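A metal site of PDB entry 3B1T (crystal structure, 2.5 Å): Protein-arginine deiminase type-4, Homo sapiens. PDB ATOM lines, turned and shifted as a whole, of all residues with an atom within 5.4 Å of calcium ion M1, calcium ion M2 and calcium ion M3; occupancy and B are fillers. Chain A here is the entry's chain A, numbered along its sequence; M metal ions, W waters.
Calcium ion M2 is bound by the side-chain carboxylate (OD2) of Asp 184, the side-chain carboxylate (OD1) of Asp 163, the side-chain carboxylate (OD2) of Asp 173, the side-chain carboxylate (OD2) of Asp 187, the side-chain carboxylate (OD2) of Asp 165 and the side-chain amide oxygen (OD1) of Asn 161.
The side-chain carboxylate of Asp 396 is in salt-bridge range of the side-chain amino group of Lys 370 (2.8 Å). The backbone carbonyl oxygen of Asp 176 lies within hydrogen-bond range of the guanidinium group of Arg 220, 2.8 Å away. The backbone carbonyl oxygen of Asn 161 lies within hydrogen-bond range of the side-chain sulfur of Cys 174 (3.3 Å). The side-chain amide nitrogen (ND2) of Asn 161 lies within hydrogen-bond range of the side-chain carboxylate (OE1) of Glu 260, at 2.5 Å.
Calcium ion M1 is bound by OD1 of Asp 396 (2.3 Å), OD2 of Asp 163 (2.3 Å), OD2 of Asp 187 (2.4 Å), OD2 of Asp 165 (2.4 Å), OD1 of Asp 165 (2.4 Å) and water W1 (2.6 Å). Calcium ion M1 has six donor atoms within binding distance. Slightly farther from calcium ion M1 lies OD1 of Asp 187 (3.1 Å).
Within 4 Å of calcium ion M2: Asn 161, Asp 163, Asp 165, Asp 173, Asp 184 and Asp 187. Along chain A the residues within 4 Å of calcium ion M2 span positions 161 to 187.
O of Asp 173 binds calcium ion M3 (2.3 Å). Calcium ion M3 is bound by O of Glu 178 (2.3 Å). OD2 of Asp 176 binds calcium ion M3, 2.4 Å away.
Three residues have an atom within 4 Å of calcium ion M3: Asp 173, Asp 176 and Glu 178. The nearest printed residue that does not touch calcium ion M3 is Cys 174 (4.2 Å).
Of the 21 residues printed, 4 come within 4 Å of calcium ion M1.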
ATOM      1  N   ASN A 161      -7.045 -18.553  30.504  1.00  0.00           N
ATOM      2  CA  ASN A 161      -7.098 -18.799  29.080  1.00  0.00           C
ATOM      3  C   ASN A 161      -5.689 -19.009  28.537  1.00  0.00           C
ATOM      4  O   ASN A 161      -5.153 -18.248  27.724  1.00  0.00           O
ATOM      5  CB  ASN A 161      -7.831 -17.635  28.414  1.00  0.00           C
ATOM      6  CG  ASN A 161      -8.118 -17.860  26.935  1.00  0.00           C
ATOM      7  OD1 ASN A 161      -8.242 -19.011  26.423  1.00  0.00           O
ATOM      8  ND2 ASN A 161      -8.230 -16.756  26.229  1.00  0.00           N
ATOM      9  N   ASP A 163      -4.398 -21.731  26.996  1.00  0.00           N
ATOM     10  CA  ASP A 163      -4.185 -22.606  25.842  1.00  0.00           C
ATOM     11  C   ASP A 163      -3.865 -21.754  24.603  1.00  0.00           C
ATOM     12  O   ASP A 163      -3.743 -20.527  24.715  1.00  0.00           O
ATOM     13  CB  ASP A 163      -5.402 -23.519  25.626  1.00  0.00           C
ATOM     14  CG  ASP A 163      -6.575 -22.811  24.957  1.00  0.00           C
ATOM     15  OD1 ASP A 163      -6.777 -21.597  25.206  1.00  0.00           O
ATOM     16  OD2 ASP A 163      -7.299 -23.468  24.178  1.00  0.00           O
ATOM     17  N   ARG A 164      -3.714 -22.418  23.451  1.00  0.00           N
ATOM     18  CA  ARG A 164      -3.341 -21.753  22.193  1.00  0.00           C
ATOM     19  C   ARG A 164      -4.235 -22.192  21.009  1.00  0.00           C
ATOM     20  O   ARG A 164      -3.845 -23.047  20.205  1.00  0.00           O
ATOM     21  CB  ARG A 164      -1.856 -22.008  21.875  1.00  0.00           C
ATOM     22  CG  ARG A 164      -1.312 -21.200  20.696  1.00  0.00           C
ATOM     23  CD  ARG A 164       0.183 -21.411  20.482  1.00  0.00           C
ATOM     24  NE  ARG A 164       0.464 -22.495  19.515  1.00  0.00           N
ATOM     25  CZ  ARG A 164       1.194 -23.583  19.757  1.00  0.00           C
ATOM     26  NH1 ARG A 164       1.768 -23.809  20.951  1.00  0.00           N
ATOM     27  NH2 ARG A 164       1.371 -24.485  18.781  1.00  0.00           N
ATOM     28  N   ASP A 165      -5.413 -21.575  20.916  1.00  0.00           N
ATOM     29  CA  ASP A 165      -6.356 -21.813  19.816  1.00  0.00           C
ATOM     30  C   ASP A 165      -5.933 -21.064  18.524  1.00  0.00           C
ATOM     31  O   ASP A 165      -6.497 -21.316  17.451  1.00  0.00           O
ATOM     32  CB  ASP A 165      -7.790 -21.405  20.213  1.00  0.00           C
ATOM     33  CG  ASP A 165      -8.335 -22.183  21.419  1.00  0.00           C
ATOM     34  OD1 ASP A 165      -8.409 -23.434  21.367  1.00  0.00           O
ATOM     35  OD2 ASP A 165      -8.710 -21.549  22.439  1.00  0.00           O
ATOM     36  N   ASP A 173      -3.039 -17.556  24.364  1.00  0.00           N
ATOM     37  CA  ASP A 173      -4.123 -16.623  23.979  1.00  0.00           C
ATOM     38  C   ASP A 173      -4.191 -15.340  24.863  1.00  0.00           C
ATOM     39  O   ASP A 173      -4.364 -14.240  24.335  1.00  0.00           O
ATOM     40  CB  ASP A 173      -5.486 -17.335  24.012  1.00  0.00           C
ATOM     41  CG  ASP A 173      -5.630 -18.459  22.976  1.00  0.00           C
ATOM     42  OD1 ASP A 173      -4.856 -18.511  21.984  1.00  0.00           O
ATOM     43  OD2 ASP A 173      -6.534 -19.312  23.145  1.00  0.00           O
ATOM     44  N   CYS A 174      -4.061 -15.498  26.189  1.00  0.00           N
ATOM     45  CA  CYS A 174      -4.224 -14.399  27.177  1.00  0.00           C
ATOM     46  C   CYS A 174      -3.051 -13.404  27.327  1.00  0.00           C
ATOM     47  O   CYS A 174      -3.152 -12.409  28.055  1.00  0.00           O
ATOM     48  CB  CYS A 174      -4.585 -14.973  28.567  1.00  0.00           C
ATOM     49  SG  CYS A 174      -3.321 -16.032  29.349  1.00  0.00           S
ATOM     50  N   GLU A 175      -1.948 -13.655  26.610  1.00  0.00           N
ATOM     51  CA  GLU A 175      -0.811 -12.725  26.612  1.00  0.00           C
ATOM     52  C   GLU A 175      -1.111 -11.387  25.910  1.00  0.00           C
ATOM     53  O   GLU A 175      -0.342 -10.438  26.044  1.00  0.00           O
ATOM     54  CB  GLU A 175       0.436 -13.391  25.997  1.00  0.00           C
ATOM     55  CG  GLU A 175       0.990 -14.532  26.839  1.00  0.00           C
ATOM     56  CD  GLU A 175       2.457 -14.848  26.544  1.00  0.00           C
ATOM     57  OE1 GLU A 175       3.013 -14.279  25.583  1.00  0.00           O
ATOM     58  OE2 GLU A 175       3.044 -15.672  27.279  1.00  0.00           O
ATOM     59  N   ASP A 176      -2.216 -11.329  25.167  1.00  0.00           N
ATOM     60  CA  ASP A 176      -2.627 -10.093  24.485  1.00  0.00           C
ATOM     61  C   ASP A 176      -4.096  -9.707  24.777  1.00  0.00           C
ATOM     62  O   ASP A 176      -4.878 -10.520  25.289  1.00  0.00           O
ATOM     63  CB  ASP A 176      -2.378 -10.210  22.978  1.00  0.00           C
ATOM     64  CG  ASP A 176      -3.250 -11.269  22.312  1.00  0.00           C
ATOM     65  OD1 ASP A 176      -2.816 -11.809  21.262  1.00  0.00           O
ATOM     66  OD2 ASP A 176      -4.352 -11.579  22.809  1.00  0.00           O
ATOM     67  N   ASP A 177      -4.430  -8.479  24.404  1.00  0.00           N
ATOM     68  CA  ASP A 177      -5.763  -7.888  24.685  1.00  0.00           C
ATOM     69  C   ASP A 177      -6.702  -7.974  23.468  1.00  0.00           C
ATOM     70  O   ASP A 177      -7.455  -7.043  23.171  1.00  0.00           O
ATOM     71  CB  ASP A 177      -5.614  -6.437  25.192  1.00  0.00           C
ATOM     72  CG  ASP A 177      -4.540  -5.646  24.437  1.00  0.00           C
ATOM     73  OD1 ASP A 177      -4.807  -5.196  23.303  1.00  0.00           O
ATOM     74  OD2 ASP A 177      -3.439  -5.460  24.983  1.00  0.00           O
ATOM     75  N   GLU A 178      -6.680  -9.134  22.801  1.00  0.00           N
ATOM     76  CA  GLU A 178      -7.406  -9.347  21.546  1.00  0.00           C
ATOM     77  C   GLU A 178      -8.020 -10.761  21.488  1.00  0.00           C
ATOM     78  O   GLU A 178      -7.410 -11.742  21.933  1.00  0.00           O
ATOM     79  CB  GLU A 178      -6.479  -9.119  20.330  1.00  0.00           C
ATOM     80  CG  GLU A 178      -5.758  -7.741  20.297  1.00  0.00           C
ATOM     81  CD  GLU A 178      -4.846  -7.557  19.079  1.00  0.00           C
ATOM     82  OE1 GLU A 178      -4.649  -8.530  18.318  1.00  0.00           O
ATOM     83  OE2 GLU A 178      -4.320  -6.439  18.882  1.00  0.00           O
ATOM     84  N   VAL A 179      -9.240 -10.849  20.937  1.00  0.00           N
ATOM     85  CA  VAL A 179      -9.891 -12.125  20.653  1.00  0.00           C
ATOM     86  C   VAL A 179      -9.819 -12.345  19.139  1.00  0.00           C
ATOM     87  O   VAL A 179     -10.528 -11.677  18.377  1.00  0.00           O
ATOM     88  CB  VAL A 179     -11.387 -12.139  21.076  1.00  0.00           C
ATOM     89  CG1 VAL A 179     -11.976 -13.523  20.864  1.00  0.00           C
ATOM     90  CG2 VAL A 179     -11.534 -11.728  22.507  1.00  0.00           C
ATOM     91  N   GLU A 183     -13.453 -19.359  18.173  1.00  0.00           N
ATOM     92  CA  GLU A 183     -13.169 -20.555  18.959  1.00  0.00           C
ATOM     93  C   GLU A 183     -12.671 -20.189  20.361  1.00  0.00           C
ATOM     94  O   GLU A 183     -12.943 -20.903  21.324  1.00  0.00           O
ATOM     95  CB  GLU A 183     -12.079 -21.407  18.270  1.00  0.00           C
ATOM     96  CG  GLU A 183     -12.473 -22.046  16.945  1.00  0.00           C
ATOM     97  CD  GLU A 183     -12.222 -21.146  15.742  1.00  0.00           C
ATOM     98  OE1 GLU A 183     -11.755 -21.662  14.707  1.00  0.00           O
ATOM     99  OE2 GLU A 183     -12.507 -19.935  15.818  1.00  0.00           O
ATOM    100  N   ASP A 184     -11.927 -19.097  20.453  1.00  0.00           N
ATOM    101  CA  ASP A 184     -11.363 -18.661  21.704  1.00  0.00           C
ATOM    102  C   ASP A 184     -12.480 -18.237  22.696  1.00  0.00           C
ATOM    103  O   ASP A 184     -12.327 -18.451  23.922  1.00  0.00           O
ATOM    104  CB  ASP A 184     -10.339 -17.528  21.455  1.00  0.00           C
ATOM    105  CG  ASP A 184      -9.505 -17.193  22.702  1.00  0.00           C
ATOM    106  OD1 ASP A 184      -9.206 -15.988  22.904  1.00  0.00           O
ATOM    107  OD2 ASP A 184      -9.149 -18.109  23.479  1.00  0.00           O
ATOM    108  N   ASP A 187     -13.771 -20.690  25.504  1.00  0.00           N
ATOM    109  CA  ASP A 187     -13.006 -20.860  26.752  1.00  0.00           C
ATOM    110  C   ASP A 187     -13.397 -19.834  27.806  1.00  0.00           C
ATOM    111  O   ASP A 187     -12.997 -19.949  28.956  1.00  0.00           O
ATOM    112  CB  ASP A 187     -11.489 -20.742  26.488  1.00  0.00           C
ATOM    113  CG  ASP A 187     -10.952 -21.901  25.676  1.00  0.00           C
ATOM    114  OD1 ASP A 187     -11.318 -23.055  25.963  1.00  0.00           O
ATOM    115  OD2 ASP A 187     -10.151 -21.649  24.752  1.00  0.00           O
ATOM    116  N   ARG A 220      -9.365 -10.339  31.977  1.00  0.00           N
ATOM    117  CA  ARG A 220      -9.659  -9.515  30.817  1.00  0.00           C
ATOM    118  C   ARG A 220     -11.113  -9.716  30.375  1.00  0.00           C
ATOM    119  O   ARG A 220     -11.643 -10.839  30.450  1.00  0.00           O
ATOM    120  CB  ARG A 220      -8.700  -9.795  29.664  1.00  0.00           C
ATOM    121  CG  ARG A 220      -8.829  -8.740  28.569  1.00  0.00           C
ATOM    122  CD  ARG A 220      -7.891  -8.949  27.467  1.00  0.00           C
ATOM    123  NE  ARG A 220      -6.516  -8.661  27.854  1.00  0.00           N
ATOM    124  CZ  ARG A 220      -5.577  -9.578  28.023  1.00  0.00           C
ATOM    125  NH1 ARG A 220      -5.840 -10.865  27.851  1.00  0.00           N
ATOM    126  NH2 ARG A 220      -4.347  -9.207  28.370  1.00  0.00           N
ATOM    127  N   PHE A 222     -14.117  -8.768  27.460  1.00  0.00           N
ATOM    128  CA  PHE A 222     -14.442  -8.258  26.126  1.00  0.00           C
ATOM    129  C   PHE A 222     -15.942  -8.027  25.971  1.00  0.00           C
ATOM    130  O   PHE A 222     -16.742  -8.857  26.410  1.00  0.00           O
ATOM    131  CB  PHE A 222     -14.003  -9.246  25.036  1.00  0.00           C
ATOM    132  CG  PHE A 222     -12.589  -9.710  25.153  1.00  0.00           C
ATOM    133  CD1 PHE A 222     -12.269 -10.789  25.958  1.00  0.00           C
ATOM    134  CD2 PHE A 222     -11.568  -9.101  24.442  1.00  0.00           C
ATOM    135  CE1 PHE A 222     -10.951 -11.224  26.068  1.00  0.00           C
ATOM    136  CE2 PHE A 222     -10.252  -9.549  24.537  1.00  0.00           C
ATOM    137  CZ  PHE A 222      -9.943 -10.608  25.341  1.00  0.00           C
ATOM    138  N   GLU A 260     -12.107 -13.817  30.656  1.00  0.00           N
ATOM    139  CA  GLU A 260     -11.007 -14.793  30.806  1.00  0.00           C
ATOM    140  C   GLU A 260     -10.127 -14.389  31.954  1.00  0.00           C
ATOM    141  O   GLU A 260     -10.056 -13.225  32.275  1.00  0.00           O
ATOM    142  CB  GLU A 260     -10.118 -14.853  29.561  1.00  0.00           C
ATOM    143  CG  GLU A 260      -9.540 -13.470  29.192  1.00  0.00           C
ATOM    144  CD  GLU A 260      -8.633 -13.483  28.023  1.00  0.00           C
ATOM    145  OE1 GLU A 260      -8.624 -14.463  27.259  1.00  0.00           O
ATOM    146  OE2 GLU A 260      -7.893 -12.500  27.870  1.00  0.00           O
ATOM    147  N   LYS A 370     -16.827 -25.450  29.984  1.00  0.00           N
ATOM    148  CA  LYS A 370     -15.653 -25.908  29.262  1.00  0.00           C
ATOM    149  C   LYS A 370     -14.595 -26.604  30.142  1.00  0.00           C
ATOM    150  O   LYS A 370     -14.151 -26.051  31.158  1.00  0.00           O
ATOM    151  CB  LYS A 370     -15.017 -24.720  28.540  1.00  0.00           C
ATOM    152  CG  LYS A 370     -13.732 -25.075  27.798  1.00  0.00           C
ATOM    153  CD  LYS A 370     -13.920 -26.207  26.788  1.00  0.00           C
ATOM    154  CE  LYS A 370     -13.726 -25.753  25.351  1.00  0.00           C
ATOM    155  NZ  LYS A 370     -13.248 -26.919  24.516  1.00  0.00           N
ATOM    156  N   LEU A 372     -10.771 -28.367  29.828  1.00  0.00           N
ATOM    157  CA  LEU A 372      -9.657 -28.575  28.925  1.00  0.00           C
ATOM    158  C   LEU A 372      -8.438 -29.037  29.640  1.00  0.00           C
ATOM    159  O   LEU A 372      -8.258 -28.690  30.803  1.00  0.00           O
ATOM    160  CB  LEU A 372      -9.341 -27.317  28.112  1.00  0.00           C
ATOM    161  CG  LEU A 372      -8.787 -26.022  28.712  1.00  0.00           C
ATOM    162  CD1 LEU A 372      -7.446 -25.638  28.059  1.00  0.00           C
ATOM    163  CD2 LEU A 372      -9.786 -24.877  28.545  1.00  0.00           C
ATOM    164  N   PRO A 395      -4.348 -26.186  20.615  1.00  0.00           N
ATOM    165  CA  PRO A 395      -5.803 -26.081  20.574  1.00  0.00           C
ATOM    166  C   PRO A 395      -6.458 -27.007  21.581  1.00  0.00           C
ATOM    167  O   PRO A 395      -6.342 -28.235  21.482  1.00  0.00           O
ATOM    168  CB  PRO A 395      -6.161 -26.462  19.136  1.00  0.00           C
ATOM    169  CG  PRO A 395      -4.912 -26.255  18.353  1.00  0.00           C
ATOM    170  CD  PRO A 395      -3.801 -26.582  19.299  1.00  0.00           C
ATOM    171  N   ASP A 396      -7.146 -26.390  22.549  1.00  0.00           N
ATOM    172  CA  ASP A 396      -7.662 -27.050  23.738  1.00  0.00           C
ATOM    173  C   ASP A 396      -6.577 -27.820  24.505  1.00  0.00           C
ATOM    174  O   ASP A 396      -6.765 -28.960  24.919  1.00  0.00           O
ATOM    175  CB  ASP A 396      -8.891 -27.896  23.409  1.00  0.00           C
ATOM    176  CG  ASP A 396     -10.132 -27.047  23.137  1.00  0.00           C
ATOM    177  OD1 ASP A 396     -10.069 -25.790  23.287  1.00  0.00           O
ATOM    178  OD2 ASP A 396     -11.179 -27.634  22.773  1.00  0.00           O
HETATM  179 CA    CA M   1      -9.541 -23.550  23.492  1.00  0.00          CA
HETATM  180 CA    CA M   2      -8.392 -20.157  24.305  1.00  0.00          CA
HETATM  181 CA    CA M   3      -6.130 -13.038  23.410  1.00  0.00          CA
HETATM  182  O   HOH W   1     -11.825 -23.119  22.310  1.00  0.00           O
